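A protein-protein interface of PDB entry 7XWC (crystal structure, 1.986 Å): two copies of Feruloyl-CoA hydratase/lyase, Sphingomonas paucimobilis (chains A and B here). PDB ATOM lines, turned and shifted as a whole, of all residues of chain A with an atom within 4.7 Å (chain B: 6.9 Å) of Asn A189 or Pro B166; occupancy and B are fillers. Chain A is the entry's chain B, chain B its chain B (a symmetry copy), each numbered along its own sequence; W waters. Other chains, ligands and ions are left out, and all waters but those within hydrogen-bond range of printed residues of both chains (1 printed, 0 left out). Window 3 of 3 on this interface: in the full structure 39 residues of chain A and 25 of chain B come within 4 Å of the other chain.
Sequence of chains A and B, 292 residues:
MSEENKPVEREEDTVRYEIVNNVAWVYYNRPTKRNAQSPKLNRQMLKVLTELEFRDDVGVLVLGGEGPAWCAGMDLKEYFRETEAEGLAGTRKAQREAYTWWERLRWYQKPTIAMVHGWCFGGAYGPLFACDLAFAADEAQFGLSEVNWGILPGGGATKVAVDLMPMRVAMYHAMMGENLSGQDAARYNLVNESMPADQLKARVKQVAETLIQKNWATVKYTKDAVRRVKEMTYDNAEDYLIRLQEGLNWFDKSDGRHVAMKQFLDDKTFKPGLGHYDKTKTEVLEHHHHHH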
ATOM      1  N   LEU A 164      -1.867   6.594  24.070  1.00  0.00           N
ATOM      2  CA  LEU A 164      -2.030   5.152  24.389  1.00  0.00           C
ATOM      3  C   LEU A 164      -0.761   4.362  24.083  1.00  0.00           C
ATOM      4  O   LEU A 164      -0.548   3.304  24.775  1.00  0.00           O
ATOM      5  CB  LEU A 164      -3.193   4.557  23.594  1.00  0.00           C
ATOM      6  CG  LEU A 164      -4.568   5.148  23.901  1.00  0.00           C
ATOM      7  CD1 LEU A 164      -5.682   4.432  23.147  1.00  0.00           C
ATOM      8  CD2 LEU A 164      -4.839   5.145  25.394  1.00  0.00           C
ATOM      9  N   ALA A 185      -2.290  -4.516  18.583  1.00  0.00           N
ATOM     10  CA  ALA A 185      -3.022  -3.408  19.243  1.00  0.00           C
ATOM     11  C   ALA A 185      -3.012  -3.570  20.757  1.00  0.00           C
ATOM     12  O   ALA A 185      -2.829  -2.539  21.471  1.00  0.00           O
ATOM     13  CB  ALA A 185      -4.424  -3.305  18.724  1.00  0.00           C
ATOM     14  N   ALA A 186      -3.191  -4.806  21.229  1.00  0.00           N
ATOM     15  CA  ALA A 186      -3.160  -5.183  22.665  1.00  0.00           C
ATOM     16  C   ALA A 186      -1.733  -5.028  23.198  1.00  0.00           C
ATOM     17  O   ALA A 186      -1.548  -4.323  24.259  1.00  0.00           O
ATOM     18  CB  ALA A 186      -3.689  -6.591  22.896  1.00  0.00           C
ATOM     19  N   ARG A 187      -0.761  -5.588  22.462  1.00  0.00           N
ATOM     20  CA  ARG A 187       0.668  -5.547  22.829  1.00  0.00           C
ATOM     21  C   ARG A 187       1.087  -4.097  23.044  1.00  0.00           C
ATOM     22  O   ARG A 187       1.827  -3.859  23.945  1.00  0.00           O
ATOM     23  CB  ARG A 187       1.573  -6.130  21.755  1.00  0.00           C
ATOM     24  CG  ARG A 187       2.745  -6.883  22.341  1.00  0.00           C
ATOM     25  CD  ARG A 187       4.020  -6.715  21.556  1.00  0.00           C
ATOM     26  NE  ARG A 187       3.899  -7.027  20.143  1.00  0.00           N
ATOM     27  CZ  ARG A 187       4.743  -6.594  19.205  1.00  0.00           C
ATOM     28  NH1 ARG A 187       5.766  -5.821  19.536  1.00  0.00           N
ATOM     29  NH2 ARG A 187       4.559  -6.921  17.934  1.00  0.00           N
ATOM     30  N   TYR A 188       0.648  -3.166  22.225  1.00  0.00           N
ATOM     31  CA  TYR A 188       1.108  -1.744  22.316  1.00  0.00           C
ATOM     32  C   TYR A 188       0.086  -0.878  23.060  1.00  0.00           C
ATOM     33  O   TYR A 188       0.252   0.366  23.066  1.00  0.00           O
ATOM     34  CB  TYR A 188       1.389  -1.213  20.919  1.00  0.00           C
ATOM     35  CG  TYR A 188       2.535  -1.880  20.200  1.00  0.00           C
ATOM     36  CD1 TYR A 188       3.782  -2.027  20.795  1.00  0.00           C
ATOM     37  CD2 TYR A 188       2.383  -2.329  18.897  1.00  0.00           C
ATOM     38  CE1 TYR A 188       4.845  -2.600  20.120  1.00  0.00           C
ATOM     39  CE2 TYR A 188       3.445  -2.900  18.207  1.00  0.00           C
ATOM     40  CZ  TYR A 188       4.670  -3.040  18.824  1.00  0.00           C
ATOM     41  OH  TYR A 188       5.704  -3.600  18.132  1.00  0.00           O
ATOM     42  N   ASN A 189      -0.934  -1.508  23.647  1.00  0.00           N
ATOM     43  CA  ASN A 189      -1.874  -0.901  24.630  1.00  0.00           C
ATOM     44  C   ASN A 189      -2.757   0.145  23.979  1.00  0.00           C
ATOM     45  O   ASN A 189      -3.200   1.042  24.693  1.00  0.00           O
ATOM     46  CB  ASN A 189      -1.156  -0.282  25.832  1.00  0.00           C
ATOM     47  CG  ASN A 189      -0.147  -1.255  26.382  1.00  0.00           C
ATOM     48  OD1 ASN A 189      -0.495  -2.335  26.858  1.00  0.00           O
ATOM     49  ND2 ASN A 189       1.098  -0.913  26.211  1.00  0.00           N
ATOM     50  N   LEU A 190      -3.092  -0.041  22.712  1.00  0.00           N
ATOM     51  CA  LEU A 190      -4.172   0.705  22.010  1.00  0.00           C
ATOM     52  C   LEU A 190      -5.529   0.194  22.537  1.00  0.00           C
ATOM     53  O   LEU A 190      -6.495   0.998  22.702  1.00  0.00           O
ATOM     54  CB  LEU A 190      -3.943   0.517  20.507  1.00  0.00           C
ATOM     55  CG  LEU A 190      -4.735   1.397  19.553  1.00  0.00           C
ATOM     56  CD1 LEU A 190      -4.328   2.860  19.648  1.00  0.00           C
ATOM     57  CD2 LEU A 190      -4.556   0.903  18.129  1.00  0.00           C
ATOM     58  N   VAL A 191      -5.580  -1.103  22.837  1.00  0.00           N
ATOM     59  CA  VAL A 191      -6.734  -1.780  23.463  1.00  0.00           C
ATOM     60  C   VAL A 191      -6.228  -2.636  24.636  1.00  0.00           C
ATOM     61  O   VAL A 191      -5.019  -2.873  24.752  1.00  0.00           O
ATOM     62  CB  VAL A 191      -7.490  -2.628  22.414  1.00  0.00           C
ATOM     63  CG1 VAL A 191      -7.939  -1.788  21.242  1.00  0.00           C
ATOM     64  CG2 VAL A 191      -6.659  -3.840  21.960  1.00  0.00           C
ATOM     65  N   ALA B 161      -0.465   4.391  39.148  1.00  0.00           N
ATOM     66  CA  ALA B 161      -0.867   3.491  38.042  1.00  0.00           C
ATOM     67  C   ALA B 161      -0.676   4.197  36.696  1.00  0.00           C
ATOM     68  O   ALA B 161      -0.127   3.631  35.790  1.00  0.00           O
ATOM     69  CB  ALA B 161      -2.282   3.019  38.220  1.00  0.00           C
ATOM     70  N   VAL B 162      -1.067   5.450  36.607  1.00  0.00           N
ATOM     71  CA  VAL B 162      -0.955   6.255  35.364  1.00  0.00           C
ATOM     72  C   VAL B 162       0.497   6.615  35.026  1.00  0.00           C
ATOM     73  O   VAL B 162       0.804   6.712  33.812  1.00  0.00           O
ATOM     74  CB  VAL B 162      -1.861   7.488  35.496  1.00  0.00           C
ATOM     75  CG1 VAL B 162      -1.500   8.587  34.514  1.00  0.00           C
ATOM     76  CG2 VAL B 162      -3.297   7.061  35.322  1.00  0.00           C
ATOM     77  N   ASP B 163       1.352   6.896  35.999  1.00  0.00           N
ATOM     78  CA  ASP B 163       2.764   7.277  35.713  1.00  0.00           C
ATOM     79  C   ASP B 163       3.623   6.044  35.407  1.00  0.00           C
ATOM     80  O   ASP B 163       4.639   6.225  34.728  1.00  0.00           O
ATOM     81  CB  ASP B 163       3.352   8.146  36.829  1.00  0.00           C
ATOM     82  CG  ASP B 163       2.883   9.600  36.748  1.00  0.00           C
ATOM     83  OD1 ASP B 163       1.943   9.859  35.958  1.00  0.00           O
ATOM     84  OD2 ASP B 163       3.443  10.476  37.484  1.00  0.00           O
ATOM     85  N   LEU B 164       3.247   4.854  35.834  1.00  0.00           N
ATOM     86  CA  LEU B 164       4.076   3.650  35.572  1.00  0.00           C
ATOM     87  C   LEU B 164       3.491   2.798  34.450  1.00  0.00           C
ATOM     88  O   LEU B 164       4.312   2.091  33.763  1.00  0.00           O
ATOM     89  CB  LEU B 164       4.194   2.797  36.837  1.00  0.00           C
ATOM     90  CG  LEU B 164       4.899   3.466  38.015  1.00  0.00           C
ATOM     91  CD1 LEU B 164       5.068   2.518  39.196  1.00  0.00           C
ATOM     92  CD2 LEU B 164       6.236   4.043  37.592  1.00  0.00           C
ATOM     93  N   MET B 165       2.167   2.669  34.356  1.00  0.00           N
ATOM     94  CA  MET B 165       1.592   1.677  33.397  1.00  0.00           C
ATOM     95  C   MET B 165       0.975   2.361  32.178  1.00  0.00           C
ATOM     96  O   MET B 165       0.669   3.547  32.237  1.00  0.00           O
ATOM     97  CB  MET B 165       0.584   0.799  34.109  1.00  0.00           C
ATOM     98  CG  MET B 165       1.215   0.026  35.240  1.00  0.00           C
ATOM     99  SD  MET B 165       0.188  -1.330  35.840  1.00  0.00           S
ATOM    100  CE  MET B 165      -1.164  -0.394  36.539  1.00  0.00           C
ATOM    101  N   PRO B 166       0.776   1.644  31.037  1.00  0.00           N
ATOM    102  CA  PRO B 166       0.048   2.183  29.888  1.00  0.00           C
ATOM    103  C   PRO B 166      -1.373   2.570  30.342  1.00  0.00           C
ATOM    104  O   PRO B 166      -1.936   1.906  31.200  1.00  0.00           O
ATOM    105  CB  PRO B 166       0.026   1.044  28.857  1.00  0.00           C
ATOM    106  CG  PRO B 166       1.153   0.138  29.274  1.00  0.00           C
ATOM    107  CD  PRO B 166       1.189   0.248  30.787  1.00  0.00           C
ATOM    108  N   MET B 167      -1.858   3.705  29.849  1.00  0.00           N
ATOM    109  CA  MET B 167      -3.177   4.260  30.194  1.00  0.00           C
ATOM    110  C   MET B 167      -4.284   3.173  30.199  1.00  0.00           C
ATOM    111  O   MET B 167      -5.112   3.166  31.148  1.00  0.00           O
ATOM    112  CB  MET B 167      -3.549   5.375  29.238  1.00  0.00           C
ATOM    113  CG  MET B 167      -4.914   5.878  29.603  1.00  0.00           C
ATOM    114  SD  MET B 167      -5.382   7.246  28.567  1.00  0.00           S
ATOM    115  CE  MET B 167      -7.071   7.513  29.139  1.00  0.00           C
ATOM    116  N   ARG B 168      -4.343   2.308  29.190  1.00  0.00           N
ATOM    117  CA  ARG B 168      -5.434   1.305  29.082  1.00  0.00           C
ATOM    118  C   ARG B 168      -5.361   0.329  30.249  1.00  0.00           C
ATOM    119  O   ARG B 168      -6.411  -0.142  30.715  1.00  0.00           O
ATOM    120  CB  ARG B 168      -5.307   0.466  27.806  1.00  0.00           C
ATOM    121  CG  ARG B 168      -5.868   1.095  26.554  1.00  0.00           C
ATOM    122  CD  ARG B 168      -7.365   1.189  26.492  1.00  0.00           C
ATOM    123  NE  ARG B 168      -7.722   1.638  25.174  1.00  0.00           N
ATOM    124  CZ  ARG B 168      -8.819   2.306  24.873  1.00  0.00           C
ATOM    125  NH1 ARG B 168      -9.714   2.586  25.796  1.00  0.00           N
ATOM    126  NH2 ARG B 168      -9.041   2.641  23.622  1.00  0.00           N
ATOM    127  N   VAL B 169      -4.138  -0.028  30.645  1.00  0.00           N
ATOM    128  CA  VAL B 169      -3.887  -0.944  31.780  1.00  0.00           C
ATOM    129  C   VAL B 169      -4.263  -0.237  33.077  1.00  0.00           C
ATOM    130  O   VAL B 169      -4.944  -0.826  33.927  1.00  0.00           O
ATOM    131  CB  VAL B 169      -2.442  -1.456  31.736  1.00  0.00           C
ATOM    132  CG1 VAL B 169      -2.173  -2.384  32.891  1.00  0.00           C
ATOM    133  CG2 VAL B 169      -2.186  -2.171  30.420  1.00  0.00           C
ATOM    134  N   ALA B 170      -3.879   1.021  33.243  1.00  0.00           N
ATOM    135  CA  ALA B 170      -4.185   1.749  34.485  1.00  0.00           C
ATOM    136  C   ALA B 170      -5.699   1.818  34.610  1.00  0.00           C
ATOM    137  O   ALA B 170      -6.203   1.644  35.684  1.00  0.00           O
ATOM    138  CB  ALA B 170      -3.591   3.137  34.504  1.00  0.00           C
ATOM    139  N   MET B 171      -6.384   2.074  33.518  1.00  0.00           N
ATOM    140  CA  MET B 171      -7.862   2.251  33.522  1.00  0.00           C
ATOM    141  C   MET B 171      -8.536   0.945  33.987  1.00  0.00           C
ATOM    142  O   MET B 171      -9.371   1.003  34.860  1.00  0.00           O
ATOM    143  CB  MET B 171      -8.332   2.625  32.120  1.00  0.00           C
ATOM    144  CG  MET B 171      -9.816   2.958  32.046  1.00  0.00           C
ATOM    145  SD  MET B 171     -10.312   4.434  32.984  1.00  0.00           S
ATOM    146  CE  MET B 171      -9.914   5.719  31.814  1.00  0.00           C
ATOM    147  N   ARG B 187       5.585  -7.002  33.348  1.00  0.00           N
ATOM    148  CA  ARG B 187       5.183  -6.826  31.938  1.00  0.00           C
ATOM    149  C   ARG B 187       4.661  -5.408  31.740  1.00  0.00           C
ATOM    150  O   ARG B 187       4.952  -4.842  30.736  1.00  0.00           O
ATOM    151  CB  ARG B 187       4.081  -7.784  31.513  1.00  0.00           C
ATOM    152  CG  ARG B 187       4.250  -8.255  30.087  1.00  0.00           C
ATOM    153  CD  ARG B 187       2.948  -8.409  29.347  1.00  0.00           C
ATOM    154  NE  ARG B 187       1.970  -9.244  30.020  1.00  0.00           N
ATOM    155  CZ  ARG B 187       0.659  -9.212  29.774  1.00  0.00           C
ATOM    156  NH1 ARG B 187       0.173  -8.375  28.872  1.00  0.00           N
ATOM    157  NH2 ARG B 187      -0.168 -10.006  30.439  1.00  0.00           N
ATOM    158  N   TYR B 188       3.890  -4.866  32.659  1.00  0.00           N
ATOM    159  CA  TYR B 188       3.257  -3.522  32.475  1.00  0.00           C
ATOM    160  C   TYR B 188       4.052  -2.432  33.200  1.00  0.00           C
ATOM    161  O   TYR B 188       3.552  -1.283  33.280  1.00  0.00           O
ATOM    162  CB  TYR B 188       1.811  -3.575  32.943  1.00  0.00           C
ATOM    163  CG  TYR B 188       0.909  -4.473  32.134  1.00  0.00           C
ATOM    164  CD1 TYR B 188       0.843  -4.382  30.749  1.00  0.00           C
ATOM    165  CD2 TYR B 188       0.083  -5.392  32.762  1.00  0.00           C
ATOM    166  CE1 TYR B 188      -0.016  -5.176  30.010  1.00  0.00           C
ATOM    167  CE2 TYR B 188      -0.789  -6.189  32.031  1.00  0.00           C
ATOM    168  CZ  TYR B 188      -0.829  -6.084  30.657  1.00  0.00           C
ATOM    169  OH  TYR B 188      -1.692  -6.872  29.953  1.00  0.00           O
ATOM    170  N   ASN B 189       5.230  -2.781  33.721  1.00  0.00           N
ATOM    171  CA  ASN B 189       6.267  -1.836  34.221  1.00  0.00           C
ATOM    172  C   ASN B 189       5.806  -1.122  35.476  1.00  0.00           C
ATOM    173  O   ASN B 189       6.289  -0.016  35.713  1.00  0.00           O
ATOM    174  CB  ASN B 189       6.684  -0.803  33.173  1.00  0.00           C
ATOM    175  CG  ASN B 189       6.978  -1.490  31.866  1.00  0.00           C
ATOM    176  OD1 ASN B 189       7.898  -2.299  31.763  1.00  0.00           O
ATOM    177  ND2 ASN B 189       6.126  -1.245  30.911  1.00  0.00           N
HETATM  178  O   HOH W   1      -2.593   2.536  26.840  1.00  0.00           O
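The backbone carbonyl oxygen (O) of Leu A190 lies within hydrogen-bond range of the guanidinium group (NE) of Arg B168, at 2.8 Å.
OD1 of Asn A189 lies close to O of Ala A186 (3.4 Å). The backbone carbonyl oxygen (O) of Ala A185 sits at hydrogen-bond distance from the backbone NH (N) of Leu A190 (2.8 Å). The backbone carbonyl oxygen of Ala A185 sits at hydrogen-bond distance from the backbone NH of Val A191.
Among the printed residues, pairs that only touch across the chains: Asn A189 with Pro B166 (3.2 Å), Asn A189 with Arg B168 (3.3 Å), Leu A164 with Arg B168 (3.8 Å), Leu A164 with Met B167 (3.8 Å), Asn A189 with Val B169 (3.9 Å) and Val A191 with Arg B168 (3.9 Å).
Of the printed residues of chain B, Leu A164 touches Met B167 (3.8 Å) and Arg B168 (3.8 Å). Asn A189 touches just these residues of chain B: Pro B166 (3.2 Å), Arg B168 (3.3 Å) and Val B169 (3.9 Å). Of chain A, only Asn A189 comes within 4 Å of Pro B166. Printed residues of chain A within 4 Å of Met B167: Leu A164 (3.8 Å). The nearest printed residue of chain A that does not touch Pro B166 is Leu A164 (4.7 Å). The nearest printed residue of chain B that does not touch Leu A164 is Pro B166 (4.7 Å).
Of the 8 printed residues of chain A, 4 touch a printed residue of chain B. Hydrophobic or aromatic side chains of chain A that line the printed part of chain B: Leu A164. Of the 14 printed residues of chain B, 4 touch a printed residue of chain A. Hydrophobic or aromatic side chains of chain B that line the printed part of chain A: Pro B166, Met B167 and Val B169. Among the printed residues, 7 pairs touch across the chains.
4 positions are printed for both chains. Of the 7 pairs that touch across the chains among the printed residues, none has its exchanged pair printed and touching as well.
Water W1 lies within hydrogen-bond range of the backbone carbonyl oxygen (O) of Asn A189 (2.7 Å), the backbone NH (N) of Arg B168 (2.9 Å), the backbone carbonyl oxygen (O) of Leu A164 (3.0 Å) and the backbone NH (N) of Met B167 (3.3 Å).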
